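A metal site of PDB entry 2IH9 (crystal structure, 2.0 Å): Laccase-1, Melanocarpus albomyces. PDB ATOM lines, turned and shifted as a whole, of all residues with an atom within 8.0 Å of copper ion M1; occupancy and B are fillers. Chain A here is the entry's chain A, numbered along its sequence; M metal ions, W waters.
N of His 434 is in hydrogen-bond range of O of His 502 (2.7 Å). N of His 436 lies within hydrogen-bond range of O of Leu 500 (2.8 Å). The side-chain carboxylate of Asp 106 is in hydrogen-bond range of a ring nitrogen (ND1) of His 436, at 2.9 Å. The chain-end carboxylate (OXT) of Leu 559 sits at hydrogen-bond distance from a ring nitrogen (ND1) of His 140 (3.0 Å).
Copper ion M1 is bound by NE2 of His 502 (1.9 Å), NE2 of His 436 (1.9 Å), NE2 of His 140 (2.0 Å) and water W1 (2.6 Å). Copper ion M1 has four donor atoms within binding distance.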
ATOM      1  N   HIS A  93     -25.768  26.474 -12.176  1.00  0.00           N
ATOM      2  CA  HIS A  93     -24.461  26.653 -11.559  1.00  0.00           C
ATOM      3  C   HIS A  93     -23.449  25.872 -12.348  1.00  0.00           C
ATOM      4  O   HIS A  93     -23.645  24.702 -12.627  1.00  0.00           O
ATOM      5  CB  HIS A  93     -24.482  26.208 -10.090  1.00  0.00           C
ATOM      6  CG  HIS A  93     -23.131  26.228  -9.424  1.00  0.00           C
ATOM      7  ND1 HIS A  93     -22.277  27.303  -9.512  1.00  0.00           N
ATOM      8  CD2 HIS A  93     -22.472  25.282  -8.729  1.00  0.00           C
ATOM      9  CE1 HIS A  93     -21.146  27.010  -8.904  1.00  0.00           C
ATOM     10  NE2 HIS A  93     -21.239  25.797  -8.416  1.00  0.00           N
ATOM     11  N   HIS A  95     -20.377  24.381 -11.887  1.00  0.00           N
ATOM     12  CA  HIS A  95     -19.503  23.747 -10.896  1.00  0.00           C
ATOM     13  C   HIS A  95     -18.101  23.485 -11.459  1.00  0.00           C
ATOM     14  O   HIS A  95     -17.929  22.671 -12.359  1.00  0.00           O
ATOM     15  CB  HIS A  95     -20.167  22.433 -10.426  1.00  0.00           C
ATOM     16  CG  HIS A  95     -19.510  21.750  -9.263  1.00  0.00           C
ATOM     17  ND1 HIS A  95     -20.235  21.167  -8.238  1.00  0.00           N
ATOM     18  CD2 HIS A  95     -18.202  21.449  -9.005  1.00  0.00           C
ATOM     19  CE1 HIS A  95     -19.405  20.543  -7.414  1.00  0.00           C
ATOM     20  NE2 HIS A  95     -18.174  20.694  -7.860  1.00  0.00           N
ATOM     21  N   ASP A 106     -22.630  33.015 -11.642  1.00  0.00           N
ATOM     22  CA  ASP A 106     -22.441  31.769 -10.866  1.00  0.00           C
ATOM     23  C   ASP A 106     -23.643  30.815 -10.775  1.00  0.00           C
ATOM     24  O   ASP A 106     -23.444  29.615 -10.581  1.00  0.00           O
ATOM     25  CB  ASP A 106     -21.922  32.114  -9.466  1.00  0.00           C
ATOM     26  CG  ASP A 106     -21.312  30.909  -8.736  1.00  0.00           C
ATOM     27  OD1 ASP A 106     -20.432  30.223  -9.309  1.00  0.00           O
ATOM     28  OD2 ASP A 106     -21.707  30.666  -7.591  1.00  0.00           O
ATOM     29  N   GLY A 107     -24.872  31.340 -10.886  1.00  0.00           N
ATOM     30  CA  GLY A 107     -26.054  30.485 -10.818  1.00  0.00           C
ATOM     31  C   GLY A 107     -26.499  30.075  -9.433  1.00  0.00           C
ATOM     32  O   GLY A 107     -27.206  29.074  -9.265  1.00  0.00           O
ATOM     33  N   ALA A 108     -26.062  30.830  -8.436  1.00  0.00           N
ATOM     34  CA  ALA A 108     -26.398  30.574  -7.048  1.00  0.00           C
ATOM     35  C   ALA A 108     -27.609  31.432  -6.700  1.00  0.00           C
ATOM     36  O   ALA A 108     -27.462  32.607  -6.385  1.00  0.00           O
ATOM     37  CB  ALA A 108     -25.196  30.919  -6.159  1.00  0.00           C
ATOM     38  N   HIS A 138     -25.266  22.177 -13.015  1.00  0.00           N
ATOM     39  CA  HIS A 138     -26.503  21.703 -12.379  1.00  0.00           C
ATOM     40  C   HIS A 138     -27.333  22.864 -11.816  1.00  0.00           C
ATOM     41  O   HIS A 138     -26.806  23.961 -11.614  1.00  0.00           O
ATOM     42  CB  HIS A 138     -26.179  20.693 -11.261  1.00  0.00           C
ATOM     43  CG  HIS A 138     -25.324  21.231 -10.157  1.00  0.00           C
ATOM     44  ND1 HIS A 138     -25.830  21.944  -9.086  1.00  0.00           N
ATOM     45  CD2 HIS A 138     -23.988  21.141  -9.932  1.00  0.00           C
ATOM     46  CE1 HIS A 138     -24.853  22.246  -8.265  1.00  0.00           C
ATOM     47  NE2 HIS A 138     -23.722  21.774  -8.742  1.00  0.00           N
ATOM     48  N   SER A 139     -28.613  22.598 -11.525  1.00  0.00           N
ATOM     49  CA  SER A 139     -29.481  23.620 -10.929  1.00  0.00           C
ATOM     50  C   SER A 139     -29.116  23.798  -9.453  1.00  0.00           C
ATOM     51  O   SER A 139     -28.500  22.915  -8.838  1.00  0.00           O
ATOM     52  CB  SER A 139     -30.952  23.237 -11.030  1.00  0.00           C
ATOM     53  OG  SER A 139     -31.808  24.224 -10.455  1.00  0.00           O
ATOM     54  N   HIS A 140     -29.455  24.954  -8.905  1.00  0.00           N
ATOM     55  CA  HIS A 140     -29.181  25.234  -7.511  1.00  0.00           C
ATOM     56  C   HIS A 140     -30.483  25.637  -6.811  1.00  0.00           C
ATOM     57  O   HIS A 140     -30.452  26.057  -5.664  1.00  0.00           O
ATOM     58  CB  HIS A 140     -28.079  26.293  -7.364  1.00  0.00           C
ATOM     59  CG  HIS A 140     -26.973  25.891  -6.430  1.00  0.00           C
ATOM     60  ND1 HIS A 140     -27.208  25.369  -5.182  1.00  0.00           N
ATOM     61  CD2 HIS A 140     -25.624  25.895  -6.582  1.00  0.00           C
ATOM     62  CE1 HIS A 140     -26.061  25.055  -4.607  1.00  0.00           C
ATOM     63  NE2 HIS A 140     -25.077  25.371  -5.442  1.00  0.00           N
ATOM     64  N   TYR A 145     -31.800  19.572  -9.244  1.00  0.00           N
ATOM     65  CA  TYR A 145     -30.870  18.789 -10.058  1.00  0.00           C
ATOM     66  C   TYR A 145     -31.048  17.263  -9.935  1.00  0.00           C
ATOM     67  O   TYR A 145     -30.617  16.505 -10.806  1.00  0.00           O
ATOM     68  CB  TYR A 145     -29.407  19.292  -9.887  1.00  0.00           C
ATOM     69  CG  TYR A 145     -28.511  18.679  -8.806  1.00  0.00           C
ATOM     70  CD1 TYR A 145     -27.699  17.547  -9.086  1.00  0.00           C
ATOM     71  CD2 TYR A 145     -28.400  19.279  -7.531  1.00  0.00           C
ATOM     72  CE1 TYR A 145     -26.785  17.031  -8.120  1.00  0.00           C
ATOM     73  CE2 TYR A 145     -27.497  18.776  -6.554  1.00  0.00           C
ATOM     74  CZ  TYR A 145     -26.700  17.644  -6.868  1.00  0.00           C
ATOM     75  OH  TYR A 145     -25.852  17.129  -5.934  1.00  0.00           O
ATOM     76  N   HIS A 434     -17.760  21.567  -0.723  1.00  0.00           N
ATOM     77  CA  HIS A 434     -17.505  22.239  -1.982  1.00  0.00           C
ATOM     78  C   HIS A 434     -17.457  23.757  -1.819  1.00  0.00           C
ATOM     79  O   HIS A 434     -18.245  24.315  -1.058  1.00  0.00           O
ATOM     80  CB  HIS A 434     -18.611  21.849  -2.998  1.00  0.00           C
ATOM     81  CG  HIS A 434     -18.579  22.644  -4.277  1.00  0.00           C
ATOM     82  ND1 HIS A 434     -17.451  22.760  -5.064  1.00  0.00           N
ATOM     83  CD2 HIS A 434     -19.537  23.402  -4.871  1.00  0.00           C
ATOM     84  CE1 HIS A 434     -17.712  23.568  -6.082  1.00  0.00           C
ATOM     85  NE2 HIS A 434     -18.963  23.974  -5.982  1.00  0.00           N
ATOM     86  N   LEU A 435     -16.584  24.409  -2.591  1.00  0.00           N
ATOM     87  CA  LEU A 435     -16.429  25.868  -2.567  1.00  0.00           C
ATOM     88  C   LEU A 435     -16.634  26.475  -3.938  1.00  0.00           C
ATOM     89  O   LEU A 435     -15.997  26.071  -4.906  1.00  0.00           O
ATOM     90  CB  LEU A 435     -15.043  26.260  -2.027  1.00  0.00           C
ATOM     91  CG  LEU A 435     -14.543  27.718  -1.965  1.00  0.00           C
ATOM     92  CD1 LEU A 435     -15.483  28.628  -1.181  1.00  0.00           C
ATOM     93  CD2 LEU A 435     -13.178  27.740  -1.323  1.00  0.00           C
ATOM     94  N   HIS A 436     -17.519  27.469  -4.013  1.00  0.00           N
ATOM     95  CA  HIS A 436     -17.805  28.175  -5.269  1.00  0.00           C
ATOM     96  C   HIS A 436     -16.709  29.230  -5.476  1.00  0.00           C
ATOM     97  O   HIS A 436     -16.101  29.705  -4.511  1.00  0.00           O
ATOM     98  CB  HIS A 436     -19.172  28.883  -5.236  1.00  0.00           C
ATOM     99  CG  HIS A 436     -20.364  27.972  -5.336  1.00  0.00           C
ATOM    100  ND1 HIS A 436     -21.554  28.371  -5.906  1.00  0.00           N
ATOM    101  CD2 HIS A 436     -20.574  26.711  -4.873  1.00  0.00           C
ATOM    102  CE1 HIS A 436     -22.445  27.398  -5.791  1.00  0.00           C
ATOM    103  NE2 HIS A 436     -21.874  26.379  -5.172  1.00  0.00           N
ATOM    104  N   TRP A 499     -19.595  33.888  -2.469  1.00  0.00           N
ATOM    105  CA  TRP A 499     -19.359  32.476  -2.782  1.00  0.00           C
ATOM    106  C   TRP A 499     -19.826  31.501  -1.733  1.00  0.00           C
ATOM    107  O   TRP A 499     -19.394  31.565  -0.574  1.00  0.00           O
ATOM    108  CB  TRP A 499     -17.871  32.219  -3.058  1.00  0.00           C
ATOM    109  CG  TRP A 499     -17.225  33.176  -4.014  1.00  0.00           C
ATOM    110  CD1 TRP A 499     -16.332  34.159  -3.694  1.00  0.00           C
ATOM    111  CD2 TRP A 499     -17.470  33.292  -5.421  1.00  0.00           C
ATOM    112  NE1 TRP A 499     -16.022  34.888  -4.816  1.00  0.00           N
ATOM    113  CE2 TRP A 499     -16.698  34.385  -5.891  1.00  0.00           C
ATOM    114  CE3 TRP A 499     -18.272  32.565  -6.341  1.00  0.00           C
ATOM    115  CZ2 TRP A 499     -16.702  34.790  -7.245  1.00  0.00           C
ATOM    116  CZ3 TRP A 499     -18.276  32.970  -7.695  1.00  0.00           C
ATOM    117  CH2 TRP A 499     -17.494  34.069  -8.125  1.00  0.00           C
ATOM    118  N   LEU A 500     -20.669  30.572  -2.160  1.00  0.00           N
ATOM    119  CA  LEU A 500     -21.183  29.516  -1.304  1.00  0.00           C
ATOM    120  C   LEU A 500     -20.138  28.450  -1.037  1.00  0.00           C
ATOM    121  O   LEU A 500     -19.340  28.095  -1.936  1.00  0.00           O
ATOM    122  CB  LEU A 500     -22.411  28.850  -1.933  1.00  0.00           C
ATOM    123  CG  LEU A 500     -23.678  29.684  -2.004  1.00  0.00           C
ATOM    124  CD1 LEU A 500     -24.746  28.915  -2.774  1.00  0.00           C
ATOM    125  CD2 LEU A 500     -24.159  30.044  -0.602  1.00  0.00           C
ATOM    126  N   PHE A 501     -20.129  27.992   0.200  1.00  0.00           N
ATOM    127  CA  PHE A 501     -19.261  26.937   0.700  1.00  0.00           C
ATOM    128  C   PHE A 501     -20.253  26.021   1.405  1.00  0.00           C
ATOM    129  O   PHE A 501     -20.837  26.401   2.437  1.00  0.00           O
ATOM    130  CB  PHE A 501     -18.213  27.492   1.667  1.00  0.00           C
ATOM    131  CG  PHE A 501     -17.283  26.447   2.256  1.00  0.00           C
ATOM    132  CD1 PHE A 501     -16.471  25.660   1.418  1.00  0.00           C
ATOM    133  CD2 PHE A 501     -17.231  26.241   3.645  1.00  0.00           C
ATOM    134  CE1 PHE A 501     -15.613  24.672   1.958  1.00  0.00           C
ATOM    135  CE2 PHE A 501     -16.386  25.259   4.203  1.00  0.00           C
ATOM    136  CZ  PHE A 501     -15.567  24.473   3.353  1.00  0.00           C
ATOM    137  N   HIS A 502     -20.465  24.860   0.800  1.00  0.00           N
ATOM    138  CA  HIS A 502     -21.431  23.888   1.301  1.00  0.00           C
ATOM    139  C   HIS A 502     -21.111  22.428   1.111  1.00  0.00           C
ATOM    140  O   HIS A 502     -20.220  22.058   0.343  1.00  0.00           O
ATOM    141  CB  HIS A 502     -22.815  24.147   0.643  1.00  0.00           C
ATOM    142  CG  HIS A 502     -22.829  24.043  -0.862  1.00  0.00           C
ATOM    143  ND1 HIS A 502     -23.203  22.887  -1.523  1.00  0.00           N
ATOM    144  CD2 HIS A 502     -22.591  24.958  -1.831  1.00  0.00           C
ATOM    145  CE1 HIS A 502     -23.192  23.102  -2.824  1.00  0.00           C
ATOM    146  NE2 HIS A 502     -22.828  24.353  -3.042  1.00  0.00           N
ATOM    147  N   CYS A 503     -21.903  21.598   1.787  1.00  0.00           N
ATOM    148  CA  CYS A 503     -21.851  20.148   1.666  1.00  0.00           C
ATOM    149  C   CYS A 503     -22.634  19.935   0.379  1.00  0.00           C
ATOM    150  O   CYS A 503     -23.687  20.566   0.192  1.00  0.00           O
ATOM    151  CB  CYS A 503     -22.600  19.474   2.812  1.00  0.00           C
ATOM    152  SG  CYS A 503     -22.865  17.736   2.542  1.00  0.00           S
ATOM    153  N   HIS A 504     -22.134  19.083  -0.514  1.00  0.00           N
ATOM    154  CA  HIS A 504     -22.821  18.869  -1.775  1.00  0.00           C
ATOM    155  C   HIS A 504     -23.935  17.814  -1.754  1.00  0.00           C
ATOM    156  O   HIS A 504     -24.578  17.588  -2.789  1.00  0.00           O
ATOM    157  CB  HIS A 504     -21.818  18.605  -2.907  1.00  0.00           C
ATOM    158  CG  HIS A 504     -22.211  19.219  -4.219  1.00  0.00           C
ATOM    159  ND1 HIS A 504     -23.243  18.738  -4.997  1.00  0.00           N
ATOM    160  CD2 HIS A 504     -21.666  20.247  -4.916  1.00  0.00           C
ATOM    161  CE1 HIS A 504     -23.310  19.432  -6.128  1.00  0.00           C
ATOM    162  NE2 HIS A 504     -22.353  20.347  -6.105  1.00  0.00           N
ATOM    163  N   VAL A 509     -27.505  20.343   2.186  1.00  0.00           N
ATOM    164  CA  VAL A 509     -27.534  21.770   1.821  1.00  0.00           C
ATOM    165  C   VAL A 509     -28.968  22.312   1.926  1.00  0.00           C
ATOM    166  O   VAL A 509     -29.171  23.465   2.358  1.00  0.00           O
ATOM    167  CB  VAL A 509     -26.841  22.069   0.430  1.00  0.00           C
ATOM    168  CG1 VAL A 509     -27.562  21.385  -0.735  1.00  0.00           C
ATOM    169  CG2 VAL A 509     -26.743  23.578   0.191  1.00  0.00           C
ATOM    170  N   SER A 514     -24.539  25.188   4.922  1.00  0.00           N
ATOM    171  CA  SER A 514     -23.811  26.117   4.064  1.00  0.00           C
ATOM    172  C   SER A 514     -23.496  27.434   4.718  1.00  0.00           C
ATOM    173  O   SER A 514     -24.132  27.812   5.717  1.00  0.00           O
ATOM    174  CB  SER A 514     -24.577  26.414   2.765  1.00  0.00           C
ATOM    175  OG  SER A 514     -23.825  27.246   1.899  1.00  0.00           O
ATOM    176  N   LEU A 559     -31.367  26.186  -1.502  1.00  0.00           N
ATOM    177  CA  LEU A 559     -30.080  25.857  -2.139  1.00  0.00           C
ATOM    178  C   LEU A 559     -29.880  24.364  -2.356  1.00  0.00           C
ATOM    179  O   LEU A 559     -30.456  23.594  -1.567  1.00  0.00           O
ATOM    180  CB  LEU A 559     -28.918  26.407  -1.310  1.00  0.00           C
ATOM    181  CG  LEU A 559     -28.724  27.923  -1.183  1.00  0.00           C
ATOM    182  CD1 LEU A 559     -27.553  28.234  -0.266  1.00  0.00           C
ATOM    183  CD2 LEU A 559     -28.533  28.556  -2.533  1.00  0.00           C
ATOM    184  OXT LEU A 559     -29.172  23.979  -3.312  1.00  0.00           O
HETATM  185 CU    CU M   1     -23.238  25.111  -4.746  1.00  0.00          CU
HETATM  186 CU    CU M   2     -20.074  24.803  -7.296  1.00  0.00          CU
HETATM  187 CU    CU M   3     -22.094  21.449  -7.739  1.00  0.00          CU
HETATM  188  O   HOH W   1     -22.975  23.070  -6.327  1.00  0.00           O
